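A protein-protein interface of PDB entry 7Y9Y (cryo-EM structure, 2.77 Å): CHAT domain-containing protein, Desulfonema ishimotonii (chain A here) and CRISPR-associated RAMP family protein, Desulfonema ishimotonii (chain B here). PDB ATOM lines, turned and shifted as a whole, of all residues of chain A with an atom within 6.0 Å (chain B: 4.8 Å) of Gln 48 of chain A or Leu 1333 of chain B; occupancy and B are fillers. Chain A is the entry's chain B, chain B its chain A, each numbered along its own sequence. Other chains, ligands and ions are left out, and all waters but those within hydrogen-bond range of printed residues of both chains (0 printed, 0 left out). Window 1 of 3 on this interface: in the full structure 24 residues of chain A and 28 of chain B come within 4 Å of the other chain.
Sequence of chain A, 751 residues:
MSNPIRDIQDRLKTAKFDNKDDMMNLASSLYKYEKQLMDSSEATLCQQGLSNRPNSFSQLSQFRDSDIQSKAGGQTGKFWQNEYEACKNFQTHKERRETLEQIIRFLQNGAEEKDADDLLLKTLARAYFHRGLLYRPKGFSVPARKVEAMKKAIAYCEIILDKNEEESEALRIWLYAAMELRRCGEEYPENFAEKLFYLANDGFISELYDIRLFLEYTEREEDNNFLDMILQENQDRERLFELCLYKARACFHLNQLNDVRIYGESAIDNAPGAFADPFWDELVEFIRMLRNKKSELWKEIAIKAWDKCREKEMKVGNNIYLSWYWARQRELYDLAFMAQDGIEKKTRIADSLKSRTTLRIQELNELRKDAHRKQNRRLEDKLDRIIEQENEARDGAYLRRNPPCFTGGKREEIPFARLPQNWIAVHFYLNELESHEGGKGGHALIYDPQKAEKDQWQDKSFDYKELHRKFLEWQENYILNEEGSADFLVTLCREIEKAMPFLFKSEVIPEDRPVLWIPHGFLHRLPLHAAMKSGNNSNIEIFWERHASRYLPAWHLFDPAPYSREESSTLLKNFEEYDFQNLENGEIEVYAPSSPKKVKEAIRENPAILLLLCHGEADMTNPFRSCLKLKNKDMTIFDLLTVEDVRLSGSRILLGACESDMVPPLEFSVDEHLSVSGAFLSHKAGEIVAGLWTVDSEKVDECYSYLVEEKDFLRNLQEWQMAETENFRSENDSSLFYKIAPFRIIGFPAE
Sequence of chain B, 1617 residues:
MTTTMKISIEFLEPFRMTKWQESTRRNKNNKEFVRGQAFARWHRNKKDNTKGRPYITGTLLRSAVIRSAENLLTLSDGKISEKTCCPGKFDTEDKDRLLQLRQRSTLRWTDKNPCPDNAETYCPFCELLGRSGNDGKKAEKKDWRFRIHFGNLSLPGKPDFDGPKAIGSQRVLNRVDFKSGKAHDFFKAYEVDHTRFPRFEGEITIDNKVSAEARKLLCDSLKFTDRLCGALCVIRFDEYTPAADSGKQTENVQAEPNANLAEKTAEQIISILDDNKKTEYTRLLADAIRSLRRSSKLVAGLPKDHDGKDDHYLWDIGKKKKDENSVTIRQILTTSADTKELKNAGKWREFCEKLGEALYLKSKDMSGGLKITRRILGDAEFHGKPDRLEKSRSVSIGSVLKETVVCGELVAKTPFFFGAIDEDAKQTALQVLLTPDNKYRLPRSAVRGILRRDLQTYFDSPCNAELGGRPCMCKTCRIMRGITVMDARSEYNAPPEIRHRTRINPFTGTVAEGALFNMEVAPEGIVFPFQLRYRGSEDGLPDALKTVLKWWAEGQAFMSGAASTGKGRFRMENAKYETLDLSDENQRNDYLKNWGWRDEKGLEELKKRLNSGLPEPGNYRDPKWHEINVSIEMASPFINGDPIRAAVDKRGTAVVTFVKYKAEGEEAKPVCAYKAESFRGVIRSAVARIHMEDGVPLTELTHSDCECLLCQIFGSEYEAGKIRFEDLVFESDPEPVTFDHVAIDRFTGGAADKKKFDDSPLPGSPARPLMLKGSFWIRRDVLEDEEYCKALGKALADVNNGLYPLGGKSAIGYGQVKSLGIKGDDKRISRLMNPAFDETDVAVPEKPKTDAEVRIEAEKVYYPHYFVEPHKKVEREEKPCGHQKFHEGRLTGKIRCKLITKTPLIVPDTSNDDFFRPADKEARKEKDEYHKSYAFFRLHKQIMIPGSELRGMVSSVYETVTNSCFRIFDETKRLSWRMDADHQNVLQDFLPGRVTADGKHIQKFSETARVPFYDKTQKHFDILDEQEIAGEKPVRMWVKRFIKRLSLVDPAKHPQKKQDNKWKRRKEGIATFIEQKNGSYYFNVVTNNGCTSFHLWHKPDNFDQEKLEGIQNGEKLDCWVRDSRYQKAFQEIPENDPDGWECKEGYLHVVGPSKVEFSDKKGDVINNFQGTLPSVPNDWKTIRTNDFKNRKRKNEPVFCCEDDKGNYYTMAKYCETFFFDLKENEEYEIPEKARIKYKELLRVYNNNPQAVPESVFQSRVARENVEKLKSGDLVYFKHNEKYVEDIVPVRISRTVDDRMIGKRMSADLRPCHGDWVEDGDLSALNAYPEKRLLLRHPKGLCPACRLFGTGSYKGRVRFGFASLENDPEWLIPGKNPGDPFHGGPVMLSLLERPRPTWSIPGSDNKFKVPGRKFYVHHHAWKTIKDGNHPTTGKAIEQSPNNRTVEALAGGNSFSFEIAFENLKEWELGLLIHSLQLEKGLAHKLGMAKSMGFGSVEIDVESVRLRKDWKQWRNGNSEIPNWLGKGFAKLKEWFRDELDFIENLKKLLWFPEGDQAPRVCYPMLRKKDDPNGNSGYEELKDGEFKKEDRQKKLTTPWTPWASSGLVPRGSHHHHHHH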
ATOM      1  N   ASN A   3      15.034  18.252   0.999  1.00  0.00           N
ATOM      2  CA  ASN A   3      14.411  17.272   1.882  1.00  0.00           C
ATOM      3  C   ASN A   3      13.009  16.928   1.398  1.00  0.00           C
ATOM      4  O   ASN A   3      12.030  17.512   1.860  1.00  0.00           O
ATOM      5  CB  ASN A   3      14.360  17.796   3.317  1.00  0.00           C
ATOM      6  CG  ASN A   3      14.544  16.697   4.346  1.00  0.00           C
ATOM      7  OD1 ASN A   3      15.661  16.420   4.780  1.00  0.00           O
ATOM      8  ND2 ASN A   3      13.446  16.064   4.739  1.00  0.00           N
ATOM      9  N   PRO A   4      12.915  15.983   0.459  1.00  0.00           N
ATOM     10  CA  PRO A   4      11.593  15.596  -0.059  1.00  0.00           C
ATOM     11  C   PRO A   4      10.664  15.055   1.009  1.00  0.00           C
ATOM     12  O   PRO A   4       9.446  15.248   0.914  1.00  0.00           O
ATOM     13  CB  PRO A   4      11.926  14.523  -1.105  1.00  0.00           C
ATOM     14  CG  PRO A   4      13.368  14.726  -1.432  1.00  0.00           C
ATOM     15  CD  PRO A   4      14.003  15.223  -0.176  1.00  0.00           C
ATOM     16  N   ILE A   5      11.204  14.376   2.023  1.00  0.00           N
ATOM     17  CA  ILE A   5      10.361  13.745   3.036  1.00  0.00           C
ATOM     18  C   ILE A   5       9.677  14.799   3.898  1.00  0.00           C
ATOM     19  O   ILE A   5       8.508  14.650   4.275  1.00  0.00           O
ATOM     20  CB  ILE A   5      11.194  12.762   3.877  1.00  0.00           C
ATOM     21  CG1 ILE A   5      11.929  11.791   2.951  1.00  0.00           C
ATOM     22  CG2 ILE A   5      10.303  11.999   4.840  1.00  0.00           C
ATOM     23  CD1 ILE A   5      12.779  10.772   3.663  1.00  0.00           C
ATOM     24  N   ARG A   6      10.390  15.879   4.222  1.00  0.00           N
ATOM     25  CA  ARG A   6       9.762  16.992   4.929  1.00  0.00           C
ATOM     26  C   ARG A   6       8.657  17.615   4.085  1.00  0.00           C
ATOM     27  O   ARG A   6       7.600  17.994   4.608  1.00  0.00           O
ATOM     28  CB  ARG A   6      10.819  18.035   5.298  1.00  0.00           C
ATOM     29  CG  ARG A   6      10.335  19.166   6.198  1.00  0.00           C
ATOM     30  CD  ARG A   6       9.269  18.715   7.183  1.00  0.00           C
ATOM     31  NE  ARG A   6       9.813  17.968   8.310  1.00  0.00           N
ATOM     32  CZ  ARG A   6       9.235  17.902   9.502  1.00  0.00           C
ATOM     33  NH1 ARG A   6       8.089  18.514   9.748  1.00  0.00           N
ATOM     34  NH2 ARG A   6       9.822  17.206  10.470  1.00  0.00           N
ATOM     35  N   ILE A   8       6.809  16.009   1.862  1.00  0.00           N
ATOM     36  CA  ILE A   8       5.685  15.080   1.927  1.00  0.00           C
ATOM     37  C   ILE A   8       4.960  15.221   3.256  1.00  0.00           C
ATOM     38  O   ILE A   8       3.728  15.179   3.312  1.00  0.00           O
ATOM     39  CB  ILE A   8       6.159  13.634   1.693  1.00  0.00           C
ATOM     40  CG1 ILE A   8       6.935  13.522   0.384  1.00  0.00           C
ATOM     41  CG2 ILE A   8       4.975  12.681   1.664  1.00  0.00           C
ATOM     42  CD1 ILE A   8       7.491  12.141   0.135  1.00  0.00           C
ATOM     43  N   TYR A  33       9.622  12.282  -4.698  1.00  0.00           N
ATOM     44  CA  TYR A  33      10.417  11.409  -3.838  1.00  0.00           C
ATOM     45  C   TYR A  33      10.740  10.092  -4.536  1.00  0.00           C
ATOM     46  O   TYR A  33      11.857   9.570  -4.413  1.00  0.00           O
ATOM     47  CB  TYR A  33       9.692  11.142  -2.521  1.00  0.00           C
ATOM     48  CG  TYR A  33      10.505  10.296  -1.568  1.00  0.00           C
ATOM     49  CD1 TYR A  33      11.787  10.675  -1.194  1.00  0.00           C
ATOM     50  CD2 TYR A  33      10.002   9.105  -1.065  1.00  0.00           C
ATOM     51  CE1 TYR A  33      12.538   9.900  -0.334  1.00  0.00           C
ATOM     52  CE2 TYR A  33      10.745   8.322  -0.204  1.00  0.00           C
ATOM     53  CZ  TYR A  33      12.014   8.725   0.159  1.00  0.00           C
ATOM     54  OH  TYR A  33      12.764   7.951   1.016  1.00  0.00           O
ATOM     55  N   LEU A  45      20.168   9.871   0.644  1.00  0.00           N
ATOM     56  CA  LEU A  45      20.723   9.848   1.989  1.00  0.00           C
ATOM     57  C   LEU A  45      19.726  10.325   3.034  1.00  0.00           C
ATOM     58  O   LEU A  45      20.111  10.546   4.186  1.00  0.00           O
ATOM     59  CB  LEU A  45      21.991  10.701   2.052  1.00  0.00           C
ATOM     60  CG  LEU A  45      23.317  10.008   1.721  1.00  0.00           C
ATOM     61  CD1 LEU A  45      24.457  11.014   1.705  1.00  0.00           C
ATOM     62  CD2 LEU A  45      23.613   8.880   2.699  1.00  0.00           C
ATOM     63  N   CYS A  46      18.460  10.494   2.655  1.00  0.00           N
ATOM     64  CA  CYS A  46      17.387  10.861   3.576  1.00  0.00           C
ATOM     65  C   CYS A  46      16.940   9.598   4.298  1.00  0.00           C
ATOM     66  O   CYS A  46      16.065   8.866   3.836  1.00  0.00           O
ATOM     67  CB  CYS A  46      16.227  11.503   2.824  1.00  0.00           C
ATOM     68  SG  CYS A  46      16.601  13.072   2.012  1.00  0.00           S
ATOM     69  N   GLN A  47      17.545   9.345   5.455  1.00  0.00           N
ATOM     70  CA  GLN A  47      17.304   8.126   6.213  1.00  0.00           C
ATOM     71  C   GLN A  47      16.231   8.289   7.277  1.00  0.00           C
ATOM     72  O   GLN A  47      16.208   7.516   8.237  1.00  0.00           O
ATOM     73  CB  GLN A  47      18.605   7.653   6.866  1.00  0.00           C
ATOM     74  CG  GLN A  47      19.777   7.634   5.903  1.00  0.00           C
ATOM     75  CD  GLN A  47      19.865   6.347   5.102  1.00  0.00           C
ATOM     76  OE1 GLN A  47      18.945   5.533   5.116  1.00  0.00           O
ATOM     77  NE2 GLN A  47      20.967   6.167   4.383  1.00  0.00           N
ATOM     78  N   GLN A  48      15.354   9.275   7.136  1.00  0.00           N
ATOM     79  CA  GLN A  48      14.340   9.537   8.145  1.00  0.00           C
ATOM     80  C   GLN A  48      13.018   8.866   7.768  1.00  0.00           C
ATOM     81  O   GLN A  48      12.859   8.297   6.683  1.00  0.00           O
ATOM     82  CB  GLN A  48      14.132  11.040   8.302  1.00  0.00           C
ATOM     83  CG  GLN A  48      13.652  11.723   7.025  1.00  0.00           C
ATOM     84  CD  GLN A  48      14.788  12.238   6.181  1.00  0.00           C
ATOM     85  OE1 GLN A  48      15.952  11.941   6.449  1.00  0.00           O
ATOM     86  NE2 GLN A  48      14.467  13.027   5.162  1.00  0.00           N
ATOM     87  N   GLY A  49      12.062   8.945   8.687  1.00  0.00           N
ATOM     88  CA  GLY A  49      10.722   8.470   8.421  1.00  0.00           C
ATOM     89  C   GLY A  49       9.704   9.583   8.505  1.00  0.00           C
ATOM     90  O   GLY A  49      10.003  10.726   8.153  1.00  0.00           O
ATOM     91  N   LEU A  50       8.503   9.270   8.985  1.00  0.00           N
ATOM     92  CA  LEU A  50       7.436  10.247   9.129  1.00  0.00           C
ATOM     93  C   LEU A  50       7.019  10.335  10.588  1.00  0.00           C
ATOM     94  O   LEU A  50       6.894   9.315  11.271  1.00  0.00           O
ATOM     95  CB  LEU A  50       6.223   9.881   8.267  1.00  0.00           C
ATOM     96  CG  LEU A  50       6.380   9.999   6.751  1.00  0.00           C
ATOM     97  CD1 LEU A  50       5.112   9.539   6.058  1.00  0.00           C
ATOM     98  CD2 LEU A  50       6.734  11.420   6.335  1.00  0.00           C
ATOM     99  N   ARG A  53       3.028   8.484  13.020  1.00  0.00           N
ATOM    100  CA  ARG A  53       2.833   7.327  12.149  1.00  0.00           C
ATOM    101  C   ARG A  53       1.375   6.914  11.963  1.00  0.00           C
ATOM    102  O   ARG A  53       1.006   6.587  10.822  1.00  0.00           O
ATOM    103  CB  ARG A  53       3.656   6.137  12.663  1.00  0.00           C
ATOM    104  CG  ARG A  53       5.141   6.406  12.826  1.00  0.00           C
ATOM    105  CD  ARG A  53       5.896   5.110  13.082  1.00  0.00           C
ATOM    106  NE  ARG A  53       7.215   5.342  13.657  1.00  0.00           N
ATOM    107  CZ  ARG A  53       8.309   5.575  12.945  1.00  0.00           C
ATOM    108  NH1 ARG A  53       8.278   5.622  11.624  1.00  0.00           N
ATOM    109  NH2 ARG A  53       9.463   5.771  13.576  1.00  0.00           N
ATOM    110  N   GLU B 878      20.052  14.179  10.505  1.00  0.00           N
ATOM    111  CA  GLU B 878      19.195  14.037   9.336  1.00  0.00           C
ATOM    112  C   GLU B 878      19.927  13.326   8.201  1.00  0.00           C
ATOM    113  O   GLU B 878      19.387  12.408   7.572  1.00  0.00           O
ATOM    114  CB  GLU B 878      18.710  15.428   8.915  1.00  0.00           C
ATOM    115  CG  GLU B 878      17.197  15.640   9.040  1.00  0.00           C
ATOM    116  CD  GLU B 878      16.398  14.573   8.330  1.00  0.00           C
ATOM    117  OE1 GLU B 878      15.233  14.308   8.710  1.00  0.00           O
ATOM    118  OE2 GLU B 878      16.931  14.047   7.338  1.00  0.00           O
ATOM    119  N   LYS B 879      21.171  13.726   7.944  1.00  0.00           N
ATOM    120  CA  LYS B 879      21.963  13.206   6.835  1.00  0.00           C
ATOM    121  C   LYS B 879      23.209  12.499   7.345  1.00  0.00           C
ATOM    122  O   LYS B 879      24.092  13.154   7.922  1.00  0.00           O
ATOM    123  CB  LYS B 879      22.353  14.341   5.887  1.00  0.00           C
ATOM    124  CG  LYS B 879      21.587  14.357   4.579  1.00  0.00           C
ATOM    125  CD  LYS B 879      20.097  14.258   4.822  1.00  0.00           C
ATOM    126  CE  LYS B 879      19.329  15.099   3.829  1.00  0.00           C
ATOM    127  NZ  LYS B 879      18.042  14.464   3.493  1.00  0.00           N
ATOM    128  N   PRO B1329       6.211   2.885  -2.429  1.00  0.00           N
ATOM    129  CA  PRO B1329       7.518   3.019  -1.762  1.00  0.00           C
ATOM    130  C   PRO B1329       7.467   3.742  -0.427  1.00  0.00           C
ATOM    131  O   PRO B1329       8.220   3.378   0.488  1.00  0.00           O
ATOM    132  CB  PRO B1329       8.350   3.794  -2.793  1.00  0.00           C
ATOM    133  CG  PRO B1329       7.347   4.599  -3.542  1.00  0.00           C
ATOM    134  CD  PRO B1329       6.084   3.778  -3.594  1.00  0.00           C
ATOM    135  N   GLU B1330       6.595   4.744  -0.273  1.00  0.00           N
ATOM    136  CA  GLU B1330       6.571   5.547   0.946  1.00  0.00           C
ATOM    137  C   GLU B1330       6.316   4.720   2.199  1.00  0.00           C
ATOM    138  O   GLU B1330       6.440   5.254   3.307  1.00  0.00           O
ATOM    139  CB  GLU B1330       5.513   6.648   0.837  1.00  0.00           C
ATOM    140  CG  GLU B1330       4.114   6.210   1.239  1.00  0.00           C
ATOM    141  CD  GLU B1330       3.354   5.541   0.111  1.00  0.00           C
ATOM    142  OE1 GLU B1330       3.993   5.089  -0.862  1.00  0.00           O
ATOM    143  OE2 GLU B1330       2.110   5.466   0.198  1.00  0.00           O
ATOM    144  N   LYS B1331       5.965   3.440   2.048  1.00  0.00           N
ATOM    145  CA  LYS B1331       5.867   2.542   3.192  1.00  0.00           C
ATOM    146  C   LYS B1331       7.158   2.499   3.994  1.00  0.00           C
ATOM    147  O   LYS B1331       7.105   2.360   5.221  1.00  0.00           O
ATOM    148  CB  LYS B1331       5.511   1.134   2.721  1.00  0.00           C
ATOM    149  CG  LYS B1331       4.467   0.438   3.564  1.00  0.00           C
ATOM    150  CD  LYS B1331       4.182  -0.953   3.028  1.00  0.00           C
ATOM    151  CE  LYS B1331       5.460  -1.755   2.860  1.00  0.00           C
ATOM    152  NZ  LYS B1331       6.103  -2.050   4.168  1.00  0.00           N
ATOM    153  N   ARG B1332       8.313   2.623   3.334  1.00  0.00           N
ATOM    154  CA  ARG B1332       9.575   2.618   4.066  1.00  0.00           C
ATOM    155  C   ARG B1332       9.650   3.790   5.037  1.00  0.00           C
ATOM    156  O   ARG B1332      10.322   3.709   6.072  1.00  0.00           O
ATOM    157  CB  ARG B1332      10.757   2.640   3.095  1.00  0.00           C
ATOM    158  CG  ARG B1332      11.219   4.028   2.688  1.00  0.00           C
ATOM    159  CD  ARG B1332      12.165   3.974   1.507  1.00  0.00           C
ATOM    160  NE  ARG B1332      11.584   3.275   0.369  1.00  0.00           N
ATOM    161  CZ  ARG B1332      12.286   2.586  -0.520  1.00  0.00           C
ATOM    162  NH1 ARG B1332      13.602   2.485  -0.433  1.00  0.00           N
ATOM    163  NH2 ARG B1332      11.652   1.983  -1.522  1.00  0.00           N
ATOM    164  N   LEU B1333       8.958   4.888   4.726  1.00  0.00           N
ATOM    165  CA  LEU B1333       8.960   6.041   5.616  1.00  0.00           C
ATOM    166  C   LEU B1333       8.109   5.813   6.855  1.00  0.00           C
ATOM    167  O   LEU B1333       8.212   6.587   7.812  1.00  0.00           O
ATOM    168  CB  LEU B1333       8.477   7.281   4.867  1.00  0.00           C
ATOM    169  CG  LEU B1333       9.319   7.629   3.640  1.00  0.00           C
ATOM    170  CD1 LEU B1333       8.771   8.850   2.927  1.00  0.00           C
ATOM    171  CD2 LEU B1333      10.769   7.828   4.037  1.00  0.00           C
ATOM    172  N   LEU B1334       7.269   4.779   6.861  1.00  0.00           N
ATOM    173  CA  LEU B1334       6.476   4.467   8.041  1.00  0.00           C
ATOM    174  C   LEU B1334       7.223   3.593   9.038  1.00  0.00           C
ATOM    175  O   LEU B1334       6.722   3.382  10.147  1.00  0.00           O
ATOM    176  CB  LEU B1334       5.171   3.785   7.629  1.00  0.00           C
ATOM    177  CG  LEU B1334       4.108   4.734   7.074  1.00  0.00           C
ATOM    178  CD1 LEU B1334       3.288   4.045   6.005  1.00  0.00           C
ATOM    179  CD2 LEU B1334       3.217   5.254   8.184  1.00  0.00           C
ATOM    180  N   LEU B1335       8.401   3.088   8.676  1.00  0.00           N
ATOM    181  CA  LEU B1335       9.198   2.242   9.554  1.00  0.00           C
ATOM    182  C   LEU B1335      10.513   2.897   9.956  1.00  0.00           C
ATOM    183  O   LEU B1335      11.364   2.235  10.559  1.00  0.00           O
ATOM    184  CB  LEU B1335       9.467   0.894   8.882  1.00  0.00           C
ATOM    185  CG  LEU B1335       8.242   0.126   8.383  1.00  0.00           C
ATOM    186  CD1 LEU B1335       8.641  -0.874   7.311  1.00  0.00           C
ATOM    187  CD2 LEU B1335       7.526  -0.569   9.529  1.00  0.00           C
ATOM    188  N   ARG B1336      10.698   4.175   9.643  1.00  0.00           N
ATOM    189  CA  ARG B1336      11.930   4.891   9.929  1.00  0.00           C
ATOM    190  C   ARG B1336      11.662   6.012  10.925  1.00  0.00           C
ATOM    191  O   ARG B1336      10.548   6.539  11.005  1.00  0.00           O
ATOM    192  CB  ARG B1336      12.542   5.458   8.645  1.00  0.00           C
ATOM    193  CG  ARG B1336      13.012   4.394   7.672  1.00  0.00           C
ATOM    194  CD  ARG B1336      13.784   4.986   6.510  1.00  0.00           C
ATOM    195  NE  ARG B1336      14.150   3.961   5.540  1.00  0.00           N
ATOM    196  CZ  ARG B1336      14.931   4.162   4.488  1.00  0.00           C
ATOM    197  NH1 ARG B1336      15.470   5.344   4.245  1.00  0.00           N
ATOM    198  NH2 ARG B1336      15.178   3.151   3.661  1.00  0.00           N
ATOM    199  N   HIS B1337      12.685   6.359  11.699  1.00  0.00           N
ATOM    200  CA  HIS B1337      12.519   7.377  12.726  1.00  0.00           C
ATOM    201  C   HIS B1337      12.523   8.768  12.097  1.00  0.00           C
ATOM    202  O   HIS B1337      13.275   9.018  11.148  1.00  0.00           O
ATOM    203  CB  HIS B1337      13.624   7.273  13.776  1.00  0.00           C
ATOM    204  CG  HIS B1337      13.395   8.136  14.977  1.00  0.00           C
ATOM    205  ND1 HIS B1337      12.555   7.769  16.005  1.00  0.00           N
ATOM    206  CD2 HIS B1337      13.881   9.356  15.305  1.00  0.00           C
ATOM    207  CE1 HIS B1337      12.540   8.722  16.919  1.00  0.00           C
ATOM    208  NE2 HIS B1337      13.335   9.696  16.518  1.00  0.00           N
ATOM    209  N   PRO B1338      11.695   9.692  12.596  1.00  0.00           N
ATOM    210  CA  PRO B1338      11.660  11.040  12.005  1.00  0.00           C
ATOM    211  C   PRO B1338      12.990  11.772  12.046  1.00  0.00           C
ATOM    212  O   PRO B1338      13.312  12.513  11.109  1.00  0.00           O
ATOM    213  CB  PRO B1338      10.599  11.756  12.852  1.00  0.00           C
ATOM    214  CG  PRO B1338       9.727  10.666  13.352  1.00  0.00           C
ATOM    215  CD  PRO B1338      10.640   9.510  13.608  1.00  0.00           C
ATOM    216  N   GLY B1340      16.153  10.631  12.074  1.00  0.00           N
ATOM    217  CA  GLY B1340      17.277  10.106  11.324  1.00  0.00           C
ATOM    218  C   GLY B1340      17.882   8.840  11.891  1.00  0.00           C
ATOM    219  O   GLY B1340      17.170   7.872  12.169  1.00  0.00           O
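The side-chain amino group (NZ) of Lys 879 of chain B sits at hydrogen-bond distance from the side-chain amide oxygen (OD1) of Asn 3 of chain A, at 3.3 Å.
O of Leu 1333 of chain B sits at hydrogen-bond distance from N of Leu 50 of chain A, at 2.9 Å.
NH1 of Arg 53 of chain A lies within hydrogen-bond range of O of Arg 1336 of chain B (2.5 Å).
O of His 1337 of chain B is in hydrogen-bond range of N of Gly 49 of chain A, at 2.7 Å.
The side-chain amino group (NZ) of Lys 879 of chain B lies within hydrogen-bond range of the side-chain sulfur (SG) of Cys 46 of chain A.
OE2 of Glu 878 of chain B lies close to OE1 of Gln 48 of chain A (2.5 Å).
O of Leu 1334 of chain B is in hydrogen-bond range of NH1 of Arg 53 of chain A (3.1 Å).
The side-chain amide nitrogen (ND2) of Asn 3 of chain A lies close to the side-chain amide nitrogen (NE2) of Gln 48 of chain A (3.2 Å).
The backbone NH (N) of Arg 6 of chain A sits close to the side-chain amide nitrogen (ND2) of Asn 3 of chain A, 3.1 Å away.
OE2 of Glu 878 of chain B touches OD1 of Asn 3 of chain A, 3.7 Å away.
CD1 of Ile 5 of chain A touches CD2 of Leu 1333 of chain B (3.6 Å).
O of Leu 45 of chain A touches CD of Lys 879 of chain B, at 3.8 Å.
Cys 46 of chain A touches Arg 1336 of chain B (O to NH1, 3.6 Å).
Gln 48 of chain A touches Leu 1333 of chain B.
Gln 48 of chain A touches His 1337 of chain B (CA to O, 3.2 Å).
Gln 48 of chain A touches Pro 1338 of chain B.
O of Leu 50 of chain A touches CG of Pro 1338 of chain B, at 3.8 Å.
Leu 1335 of chain B touches Arg 53 of chain A.
Pro 1338 of chain B touches Arg 53 of chain A.
Printed residues of chain B within 4 Å of Cys 46 of chain A: Lys 879 and Arg 1336.
Printed residues of chain B within 4 Å of Gln 47 of chain A: Arg 1336.
Gln 48 of chain A touches just these residues of chain B: Glu 878 (2.5 Å), Leu 1333 (3.4 Å), Arg 1336 (3.4 Å), His 1337 (3.2 Å) and Pro 1338 (3.3 Å).
Leu 1333 of chain B touches just these residues of chain A: Ile 5 (3.6 Å), Tyr 33 (3.6 Å), Gln 48 (3.4 Å), Gly 49 (3.2 Å), Leu 50 (2.9 Å) and Arg 53 (3.9 Å).
Printed residues of chain A within 4 Å of Leu 1334 of chain B: Arg 53.
Printed residues of chain A within 4 Å of Arg 1336 of chain B: Cys 46 (3.6 Å), Gln 47 (3.6 Å), Gln 48 (3.4 Å), Gly 49 (3.2 Å), Leu 50 (3.96 Å) and Arg 53 (2.5 Å).
The nearest residue of chain A that does not touch Leu 1333 of chain B is Ile 8 of chain A (4.5 Å).
The nearest printed residue of chain B that does not touch Tyr 33 of chain A is Arg 1332 of chain B (4.1 Å).
Hydrophobic or aromatic side chains of chain A that line the printed part of chain B: Ile 5, Tyr 33 and Leu 50.
Along chain A the printed residues that touch a printed residue of chain B span positions 3 to 53.
Hydrophobic or aromatic side chains of chain B that line the printed part of chain A: Leu 1333, Leu 1334 and Pro 1338.
Along chain B the printed residues that touch a printed residue of chain A span positions 878 to 1338.
Among the printed residues, 27 pairs touch across the chains.
Among the printed residues, no Asp or Glu carboxylate lies within 4 Å of a Lys or Arg side-chain nitrogen of the other chain.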
